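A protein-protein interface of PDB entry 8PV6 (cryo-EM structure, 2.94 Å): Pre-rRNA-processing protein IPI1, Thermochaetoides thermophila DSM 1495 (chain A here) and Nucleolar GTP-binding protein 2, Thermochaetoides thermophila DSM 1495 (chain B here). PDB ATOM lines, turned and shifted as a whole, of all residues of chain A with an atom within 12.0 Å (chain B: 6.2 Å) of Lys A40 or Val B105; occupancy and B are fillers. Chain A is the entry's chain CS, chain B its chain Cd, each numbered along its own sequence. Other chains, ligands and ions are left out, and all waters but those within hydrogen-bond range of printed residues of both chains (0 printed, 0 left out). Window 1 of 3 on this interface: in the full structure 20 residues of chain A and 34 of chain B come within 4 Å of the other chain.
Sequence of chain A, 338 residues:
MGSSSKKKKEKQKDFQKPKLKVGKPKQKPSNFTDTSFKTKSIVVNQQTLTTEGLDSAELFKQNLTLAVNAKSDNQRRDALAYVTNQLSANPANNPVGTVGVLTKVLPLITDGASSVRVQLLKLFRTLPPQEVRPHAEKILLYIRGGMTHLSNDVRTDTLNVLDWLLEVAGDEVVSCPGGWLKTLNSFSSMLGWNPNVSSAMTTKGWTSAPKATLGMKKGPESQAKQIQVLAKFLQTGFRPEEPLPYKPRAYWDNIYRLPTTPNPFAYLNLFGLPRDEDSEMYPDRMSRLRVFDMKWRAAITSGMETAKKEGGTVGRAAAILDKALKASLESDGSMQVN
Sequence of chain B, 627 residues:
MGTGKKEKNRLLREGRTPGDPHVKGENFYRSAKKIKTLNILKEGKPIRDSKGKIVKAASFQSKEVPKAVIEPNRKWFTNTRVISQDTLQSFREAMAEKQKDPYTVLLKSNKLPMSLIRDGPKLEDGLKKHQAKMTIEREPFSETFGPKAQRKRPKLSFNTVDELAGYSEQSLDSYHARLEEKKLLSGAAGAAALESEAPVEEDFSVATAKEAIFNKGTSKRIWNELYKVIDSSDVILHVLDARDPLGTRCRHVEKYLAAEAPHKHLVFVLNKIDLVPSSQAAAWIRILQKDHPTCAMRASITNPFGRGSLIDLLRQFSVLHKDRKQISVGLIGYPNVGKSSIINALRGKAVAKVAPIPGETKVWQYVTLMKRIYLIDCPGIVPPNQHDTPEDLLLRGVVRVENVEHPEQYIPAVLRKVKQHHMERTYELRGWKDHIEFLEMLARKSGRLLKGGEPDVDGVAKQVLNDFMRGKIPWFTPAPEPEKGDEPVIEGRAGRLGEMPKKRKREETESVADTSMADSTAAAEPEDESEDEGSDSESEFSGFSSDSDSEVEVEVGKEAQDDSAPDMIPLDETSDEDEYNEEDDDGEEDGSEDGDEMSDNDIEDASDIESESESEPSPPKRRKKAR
O of Val A43 lies within hydrogen-bond range of NE2 of Gln B316 (3.0 Å).
The backbone NH (N) of Leu B107 is in hydrogen-bond range of the backbone carbonyl oxygen (O) of Lys A38, 2.9 Å away.
O of Val B105 is in hydrogen-bond range of N of Lys A40 (3.2 Å).
O of Tyr B103 is in hydrogen-bond range of N of Ile A42.
Printed residues of chain A that touch a printed residue of chain B: Phe A37, Lys A38, Thr A39, Lys A40, Ser A41, Ile A42 and Val A43.
Among the printed residues, 13 pairs touch across the chains.
O of Asp B101 is in hydrogen-bond range of OG1 of Thr B104.
CD1 of Phe A37 touches CD2 of Leu B106, at 3.7 Å.
Lys A38 touches Leu B106 (O to C, 3.8 Å).
Val B105 touches Thr A39 (O to CA, 3.4 Å).
Thr A39 touches Leu B106 (CG2 to CD2, 3.8 Å).
Thr B104 touches Lys A40.
Lys A40 touches Leu B107.
CA of Ser A41 touches O of Tyr B103, 3.4 Å away.
Ile A42 touches Gln B316.
Leu B320 touches Ile A42.
Of the printed residues of chain B, Lys A40 touches Thr B104, Val B105 and Leu B107.
Val B105 touches just these residues of chain A: Thr A39 (3.4 Å) and Lys A40 (3.2 Å).
Thr B104 touches one residue of chain A.
Of chain A, only Phe A37 (3.7 Å), Lys A38 (3.8 Å) and Thr A39 (3.8 Å) come within 4 Å of Leu B106.
Of chain A, only Lys A38 and Lys A40 come within 4 Å of Leu B107.
No residue of chain A comes within 4 Å of Val B319.
Printed residues of chain B within 4 Å of Phe A37: Leu B106.
Of the printed residues of chain B, Lys A38 touches Leu B106 (3.8 Å) and Leu B107 (2.9 Å).
Of the printed residues of chain A, Tyr B103 touches Ser A41 (3.4 Å) and Ile A42 (2.8 Å).
Pro B102 touches none of the printed residues of chain A.
Val A44 touches none of the printed residues of chain B.
The nearest printed residue of chain B that does not touch Lys A40 is Tyr B103 (4.01 Å).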
ATOM      1  N   SER A  36     -32.012 -13.284  -5.187  1.00  0.00           N
ATOM      2  CA  SER A  36     -31.509 -12.434  -4.118  1.00  0.00           C
ATOM      3  C   SER A  36     -30.409 -13.148  -3.342  1.00  0.00           C
ATOM      4  O   SER A  36     -30.487 -14.352  -3.088  1.00  0.00           O
ATOM      5  CB  SER A  36     -32.644 -12.035  -3.177  1.00  0.00           C
ATOM      6  OG  SER A  36     -33.183 -13.168  -2.522  1.00  0.00           O
ATOM      7  N   PHE A  37     -29.379 -12.395  -2.965  1.00  0.00           N
ATOM      8  CA  PHE A  37     -28.254 -12.956  -2.231  1.00  0.00           C
ATOM      9  C   PHE A  37     -27.634 -11.878  -1.355  1.00  0.00           C
ATOM     10  O   PHE A  37     -27.740 -10.687  -1.655  1.00  0.00           O
ATOM     11  CB  PHE A  37     -27.206 -13.556  -3.181  1.00  0.00           C
ATOM     12  CG  PHE A  37     -26.565 -12.555  -4.108  1.00  0.00           C
ATOM     13  CD1 PHE A  37     -25.357 -11.958  -3.784  1.00  0.00           C
ATOM     14  CD2 PHE A  37     -27.162 -12.230  -5.316  1.00  0.00           C
ATOM     15  CE1 PHE A  37     -24.767 -11.046  -4.636  1.00  0.00           C
ATOM     16  CE2 PHE A  37     -26.575 -11.318  -6.172  1.00  0.00           C
ATOM     17  CZ  PHE A  37     -25.377 -10.727  -5.831  1.00  0.00           C
ATOM     18  N   LYS A  38     -26.988 -12.311  -0.277  1.00  0.00           N
ATOM     19  CA  LYS A  38     -26.290 -11.428   0.641  1.00  0.00           C
ATOM     20  C   LYS A  38     -24.809 -11.780   0.665  1.00  0.00           C
ATOM     21  O   LYS A  38     -24.433 -12.953   0.601  1.00  0.00           O
ATOM     22  CB  LYS A  38     -26.872 -11.531   2.053  1.00  0.00           C
ATOM     23  CG  LYS A  38     -28.305 -11.050   2.167  1.00  0.00           C
ATOM     24  CD  LYS A  38     -28.817 -11.182   3.591  1.00  0.00           C
ATOM     25  CE  LYS A  38     -30.272 -10.755   3.696  1.00  0.00           C
ATOM     26  NZ  LYS A  38     -30.794 -10.913   5.082  1.00  0.00           N
ATOM     27  N   THR A  39     -23.968 -10.754   0.759  1.00  0.00           N
ATOM     28  CA  THR A  39     -22.526 -10.931   0.739  1.00  0.00           C
ATOM     29  C   THR A  39     -21.906 -10.325   1.987  1.00  0.00           C
ATOM     30  O   THR A  39     -22.343  -9.280   2.476  1.00  0.00           O
ATOM     31  CB  THR A  39     -21.897 -10.291  -0.504  1.00  0.00           C
ATOM     32  OG1 THR A  39     -22.334  -8.931  -0.613  1.00  0.00           O
ATOM     33  CG2 THR A  39     -22.301 -11.050  -1.755  1.00  0.00           C
ATOM     34  N   LYS A  40     -20.877 -10.995   2.500  1.00  0.00           N
ATOM     35  CA  LYS A  40     -20.117 -10.517   3.644  1.00  0.00           C
ATOM     36  C   LYS A  40     -18.661 -10.352   3.239  1.00  0.00           C
ATOM     37  O   LYS A  40     -18.096 -11.195   2.537  1.00  0.00           O
ATOM     38  CB  LYS A  40     -20.234 -11.473   4.837  1.00  0.00           C
ATOM     39  CG  LYS A  40     -19.690 -10.911   6.139  1.00  0.00           C
ATOM     40  CD  LYS A  40     -19.903 -11.876   7.296  1.00  0.00           C
ATOM     41  CE  LYS A  40     -21.374 -12.225   7.469  1.00  0.00           C
ATOM     42  NZ  LYS A  40     -21.591 -13.176   8.593  1.00  0.00           N
ATOM     43  N   SER A  41     -18.057  -9.258   3.691  1.00  0.00           N
ATOM     44  CA  SER A  41     -16.710  -8.875   3.292  1.00  0.00           C
ATOM     45  C   SER A  41     -15.697  -9.472   4.255  1.00  0.00           C
ATOM     46  O   SER A  41     -15.792  -9.270   5.471  1.00  0.00           O
ATOM     47  CB  SER A  41     -16.564  -7.353   3.255  1.00  0.00           C
ATOM     48  OG  SER A  41     -16.746  -6.793   4.543  1.00  0.00           O
ATOM     49  N   ILE A  42     -14.731 -10.210   3.709  1.00  0.00           N
ATOM     50  CA  ILE A  42     -13.643 -10.745   4.516  1.00  0.00           C
ATOM     51  C   ILE A  42     -12.546  -9.700   4.647  1.00  0.00           C
ATOM     52  O   ILE A  42     -12.111  -9.099   3.654  1.00  0.00           O
ATOM     53  CB  ILE A  42     -13.105 -12.043   3.891  1.00  0.00           C
ATOM     54  CG1 ILE A  42     -14.260 -12.986   3.552  1.00  0.00           C
ATOM     55  CG2 ILE A  42     -12.121 -12.715   4.823  1.00  0.00           C
ATOM     56  CD1 ILE A  42     -14.987 -13.510   4.765  1.00  0.00           C
ATOM     57  N   VAL A  43     -12.095  -9.469   5.878  1.00  0.00           N
ATOM     58  CA  VAL A  43     -11.058  -8.488   6.168  1.00  0.00           C
ATOM     59  C   VAL A  43      -9.972  -9.159   7.001  1.00  0.00           C
ATOM     60  O   VAL A  43     -10.263  -9.963   7.893  1.00  0.00           O
ATOM     61  CB  VAL A  43     -11.645  -7.239   6.873  1.00  0.00           C
ATOM     62  CG1 VAL A  43     -12.389  -7.608   8.153  1.00  0.00           C
ATOM     63  CG2 VAL A  43     -10.570  -6.193   7.147  1.00  0.00           C
ATOM     64  N   VAL A  44      -8.715  -8.868   6.674  1.00  0.00           N
ATOM     65  CA  VAL A  44      -7.566  -9.390   7.403  1.00  0.00           C
ATOM     66  C   VAL A  44      -7.131  -8.338   8.414  1.00  0.00           C
ATOM     67  O   VAL A  44      -6.773  -7.216   8.040  1.00  0.00           O
ATOM     68  CB  VAL A  44      -6.414  -9.752   6.455  1.00  0.00           C
ATOM     69  CG1 VAL A  44      -5.233 -10.282   7.241  1.00  0.00           C
ATOM     70  CG2 VAL A  44      -6.875 -10.775   5.432  1.00  0.00           C
ATOM     71  N   ASN A  45      -7.160  -8.701   9.693  1.00  0.00           N
ATOM     72  CA  ASN A  45      -6.835  -7.784  10.784  1.00  0.00           C
ATOM     73  C   ASN A  45      -5.349  -7.918  11.093  1.00  0.00           C
ATOM     74  O   ASN A  45      -4.954  -8.528  12.085  1.00  0.00           O
ATOM     75  CB  ASN A  45      -7.689  -8.085  12.008  1.00  0.00           C
ATOM     76  CG  ASN A  45      -9.169  -8.064  11.701  1.00  0.00           C
ATOM     77  OD1 ASN A  45      -9.579  -7.750  10.585  1.00  0.00           O
ATOM     78  ND2 ASN A  45      -9.980  -8.420  12.688  1.00  0.00           N
ATOM     79  N   ASP B 101     -14.772  -8.472  -6.973  1.00  0.00           N
ATOM     80  CA  ASP B 101     -14.123  -8.281  -5.680  1.00  0.00           C
ATOM     81  C   ASP B 101     -13.713  -9.628  -5.099  1.00  0.00           C
ATOM     82  O   ASP B 101     -14.584 -10.479  -4.868  1.00  0.00           O
ATOM     83  CB  ASP B 101     -15.050  -7.560  -4.718  1.00  0.00           C
ATOM     84  CG  ASP B 101     -14.308  -6.621  -3.788  1.00  0.00           C
ATOM     85  OD1 ASP B 101     -14.923  -5.641  -3.321  1.00  0.00           O
ATOM     86  OD2 ASP B 101     -13.111  -6.860  -3.524  1.00  0.00           O
ATOM     87  N   PRO B 102     -12.424  -9.869  -4.847  1.00  0.00           N
ATOM     88  CA  PRO B 102     -12.001 -11.145  -4.255  1.00  0.00           C
ATOM     89  C   PRO B 102     -12.160 -11.224  -2.746  1.00  0.00           C
ATOM     90  O   PRO B 102     -11.923 -12.293  -2.173  1.00  0.00           O
ATOM     91  CB  PRO B 102     -10.521 -11.223  -4.649  1.00  0.00           C
ATOM     92  CG  PRO B 102     -10.091  -9.802  -4.699  1.00  0.00           C
ATOM     93  CD  PRO B 102     -11.275  -9.027  -5.221  1.00  0.00           C
ATOM     94  N   TYR B 103     -12.549 -10.136  -2.082  1.00  0.00           N
ATOM     95  CA  TYR B 103     -12.757 -10.136  -0.640  1.00  0.00           C
ATOM     96  C   TYR B 103     -14.233 -10.222  -0.269  1.00  0.00           C
ATOM     97  O   TYR B 103     -14.574 -10.165   0.917  1.00  0.00           O
ATOM     98  CB  TYR B 103     -12.127  -8.893  -0.009  1.00  0.00           C
ATOM     99  CG  TYR B 103     -10.615  -8.917   0.065  1.00  0.00           C
ATOM    100  CD1 TYR B 103      -9.966  -9.118   1.276  1.00  0.00           C
ATOM    101  CD2 TYR B 103      -9.836  -8.724  -1.069  1.00  0.00           C
ATOM    102  CE1 TYR B 103      -8.591  -9.138   1.354  1.00  0.00           C
ATOM    103  CE2 TYR B 103      -8.458  -8.742  -1.000  1.00  0.00           C
ATOM    104  CZ  TYR B 103      -7.843  -8.950   0.215  1.00  0.00           C
ATOM    105  OH  TYR B 103      -6.472  -8.969   0.296  1.00  0.00           O
ATOM    106  N   THR B 104     -15.117 -10.351  -1.255  1.00  0.00           N
ATOM    107  CA  THR B 104     -16.549 -10.480  -1.022  1.00  0.00           C
ATOM    108  C   THR B 104     -16.981 -11.884  -1.410  1.00  0.00           C
ATOM    109  O   THR B 104     -16.774 -12.303  -2.553  1.00  0.00           O
ATOM    110  CB  THR B 104     -17.339  -9.447  -1.828  1.00  0.00           C
ATOM    111  OG1 THR B 104     -17.108  -9.656  -3.227  1.00  0.00           O
ATOM    112  CG2 THR B 104     -16.906  -8.042  -1.456  1.00  0.00           C
ATOM    113  N   VAL B 105     -17.581 -12.602  -0.466  1.00  0.00           N
ATOM    114  CA  VAL B 105     -18.020 -13.977  -0.671  1.00  0.00           C
ATOM    115  C   VAL B 105     -19.511 -14.052  -0.364  1.00  0.00           C
ATOM    116  O   VAL B 105     -20.036 -13.243   0.413  1.00  0.00           O
ATOM    117  CB  VAL B 105     -17.222 -14.979   0.180  1.00  0.00           C
ATOM    118  CG1 VAL B 105     -15.725 -14.793  -0.019  1.00  0.00           C
ATOM    119  CG2 VAL B 105     -17.553 -14.819   1.624  1.00  0.00           C
ATOM    120  N   LEU B 106     -20.197 -14.980  -1.025  1.00  0.00           N
ATOM    121  CA  LEU B 106     -21.635 -15.131  -0.869  1.00  0.00           C
ATOM    122  C   LEU B 106     -21.989 -15.795   0.458  1.00  0.00           C
ATOM    123  O   LEU B 106     -21.190 -16.524   1.050  1.00  0.00           O
ATOM    124  CB  LEU B 106     -22.195 -15.956  -2.024  1.00  0.00           C
ATOM    125  CG  LEU B 106     -21.737 -15.479  -3.401  1.00  0.00           C
ATOM    126  CD1 LEU B 106     -21.895 -16.576  -4.439  1.00  0.00           C
ATOM    127  CD2 LEU B 106     -22.490 -14.230  -3.803  1.00  0.00           C
ATOM    128  N   LEU B 107     -23.208 -15.533   0.920  1.00  0.00           N
ATOM    129  CA  LEU B 107     -23.805 -16.252   2.037  1.00  0.00           C
ATOM    130  C   LEU B 107     -24.876 -17.203   1.519  1.00  0.00           C
ATOM    131  O   LEU B 107     -25.706 -16.817   0.690  1.00  0.00           O
ATOM    132  CB  LEU B 107     -24.415 -15.288   3.055  1.00  0.00           C
ATOM    133  CG  LEU B 107     -23.499 -14.206   3.621  1.00  0.00           C
ATOM    134  CD1 LEU B 107     -24.274 -13.317   4.575  1.00  0.00           C
ATOM    135  CD2 LEU B 107     -22.309 -14.826   4.326  1.00  0.00           C
ATOM    136  N   HIS B 265     -12.418 -21.367  -0.068  1.00  0.00           N
ATOM    137  CA  HIS B 265     -11.779 -20.064   0.082  1.00  0.00           C
ATOM    138  C   HIS B 265     -10.268 -20.215   0.173  1.00  0.00           C
ATOM    139  O   HIS B 265      -9.760 -20.845   1.102  1.00  0.00           O
ATOM    140  CB  HIS B 265     -12.305 -19.336   1.317  1.00  0.00           C
ATOM    141  CG  HIS B 265     -13.791 -19.411   1.477  1.00  0.00           C
ATOM    142  ND1 HIS B 265     -14.666 -18.867   0.562  1.00  0.00           N
ATOM    143  CD2 HIS B 265     -14.557 -19.962   2.447  1.00  0.00           C
ATOM    144  CE1 HIS B 265     -15.907 -19.082   0.961  1.00  0.00           C
ATOM    145  NE2 HIS B 265     -15.868 -19.746   2.102  1.00  0.00           N
ATOM    146  N   GLN B 316     -13.701 -15.714  11.345  1.00  0.00           N
ATOM    147  CA  GLN B 316     -14.617 -15.122  10.371  1.00  0.00           C
ATOM    148  C   GLN B 316     -15.177 -16.181   9.432  1.00  0.00           C
ATOM    149  O   GLN B 316     -16.386 -16.209   9.168  1.00  0.00           O
ATOM    150  CB  GLN B 316     -13.917 -14.027   9.565  1.00  0.00           C
ATOM    151  CG  GLN B 316     -13.465 -12.824  10.369  1.00  0.00           C
ATOM    152  CD  GLN B 316     -12.754 -11.797   9.515  1.00  0.00           C
ATOM    153  OE1 GLN B 316     -12.959 -11.735   8.305  1.00  0.00           O
ATOM    154  NE2 GLN B 316     -11.905 -10.991  10.138  1.00  0.00           N
ATOM    155  N   PHE B 317     -14.318 -17.083   8.953  1.00  0.00           N
ATOM    156  CA  PHE B 317     -14.789 -18.151   8.070  1.00  0.00           C
ATOM    157  C   PHE B 317     -15.722 -19.120   8.795  1.00  0.00           C
ATOM    158  O   PHE B 317     -16.695 -19.606   8.209  1.00  0.00           O
ATOM    159  CB  PHE B 317     -13.602 -18.895   7.464  1.00  0.00           C
ATOM    160  CG  PHE B 317     -12.953 -18.167   6.325  1.00  0.00           C
ATOM    161  CD1 PHE B 317     -13.688 -17.819   5.205  1.00  0.00           C
ATOM    162  CD2 PHE B 317     -11.613 -17.831   6.373  1.00  0.00           C
ATOM    163  CE1 PHE B 317     -13.097 -17.147   4.156  1.00  0.00           C
ATOM    164  CE2 PHE B 317     -11.017 -17.158   5.325  1.00  0.00           C
ATOM    165  CZ  PHE B 317     -11.760 -16.817   4.216  1.00  0.00           C
ATOM    166  N   VAL B 319     -17.712 -18.427  11.472  1.00  0.00           N
ATOM    167  CA  VAL B 319     -18.984 -17.733  11.661  1.00  0.00           C
ATOM    168  C   VAL B 319     -19.737 -17.654  10.338  1.00  0.00           C
ATOM    169  O   VAL B 319     -20.969 -17.759  10.294  1.00  0.00           O
ATOM    170  CB  VAL B 319     -18.739 -16.343  12.283  1.00  0.00           C
ATOM    171  CG1 VAL B 319     -19.999 -15.491  12.277  1.00  0.00           C
ATOM    172  CG2 VAL B 319     -18.231 -16.490  13.707  1.00  0.00           C
ATOM    173  N   LEU B 320     -19.001 -17.512   9.236  1.00  0.00           N
ATOM    174  CA  LEU B 320     -19.609 -17.527   7.913  1.00  0.00           C
ATOM    175  C   LEU B 320     -20.196 -18.889   7.555  1.00  0.00           C
ATOM    176  O   LEU B 320     -21.228 -18.946   6.877  1.00  0.00           O
ATOM    177  CB  LEU B 320     -18.554 -17.100   6.896  1.00  0.00           C
ATOM    178  CG  LEU B 320     -18.969 -16.659   5.503  1.00  0.00           C
ATOM    179  CD1 LEU B 320     -18.010 -15.580   5.100  1.00  0.00           C
ATOM    180  CD2 LEU B 320     -18.918 -17.806   4.515  1.00  0.00           C
ATOM    181  N   LYS B 322     -21.326 -21.096   9.845  1.00  0.00           N
ATOM    182  CA  LYS B 322     -21.964 -21.563  11.076  1.00  0.00           C
ATOM    183  C   LYS B 322     -23.039 -22.618  10.823  1.00  0.00           C
ATOM    184  O   LYS B 322     -23.406 -23.352  11.748  1.00  0.00           O
ATOM    185  CB  LYS B 322     -22.584 -20.385  11.827  1.00  0.00           C
ATOM    186  CG  LYS B 322     -23.573 -19.589  10.996  1.00  0.00           C
ATOM    187  CD  LYS B 322     -24.049 -18.346  11.722  1.00  0.00           C
ATOM    188  CE  LYS B 322     -24.960 -17.523  10.829  1.00  0.00           C
ATOM    189  NZ  LYS B 322     -25.412 -16.268  11.488  1.00  0.00           N
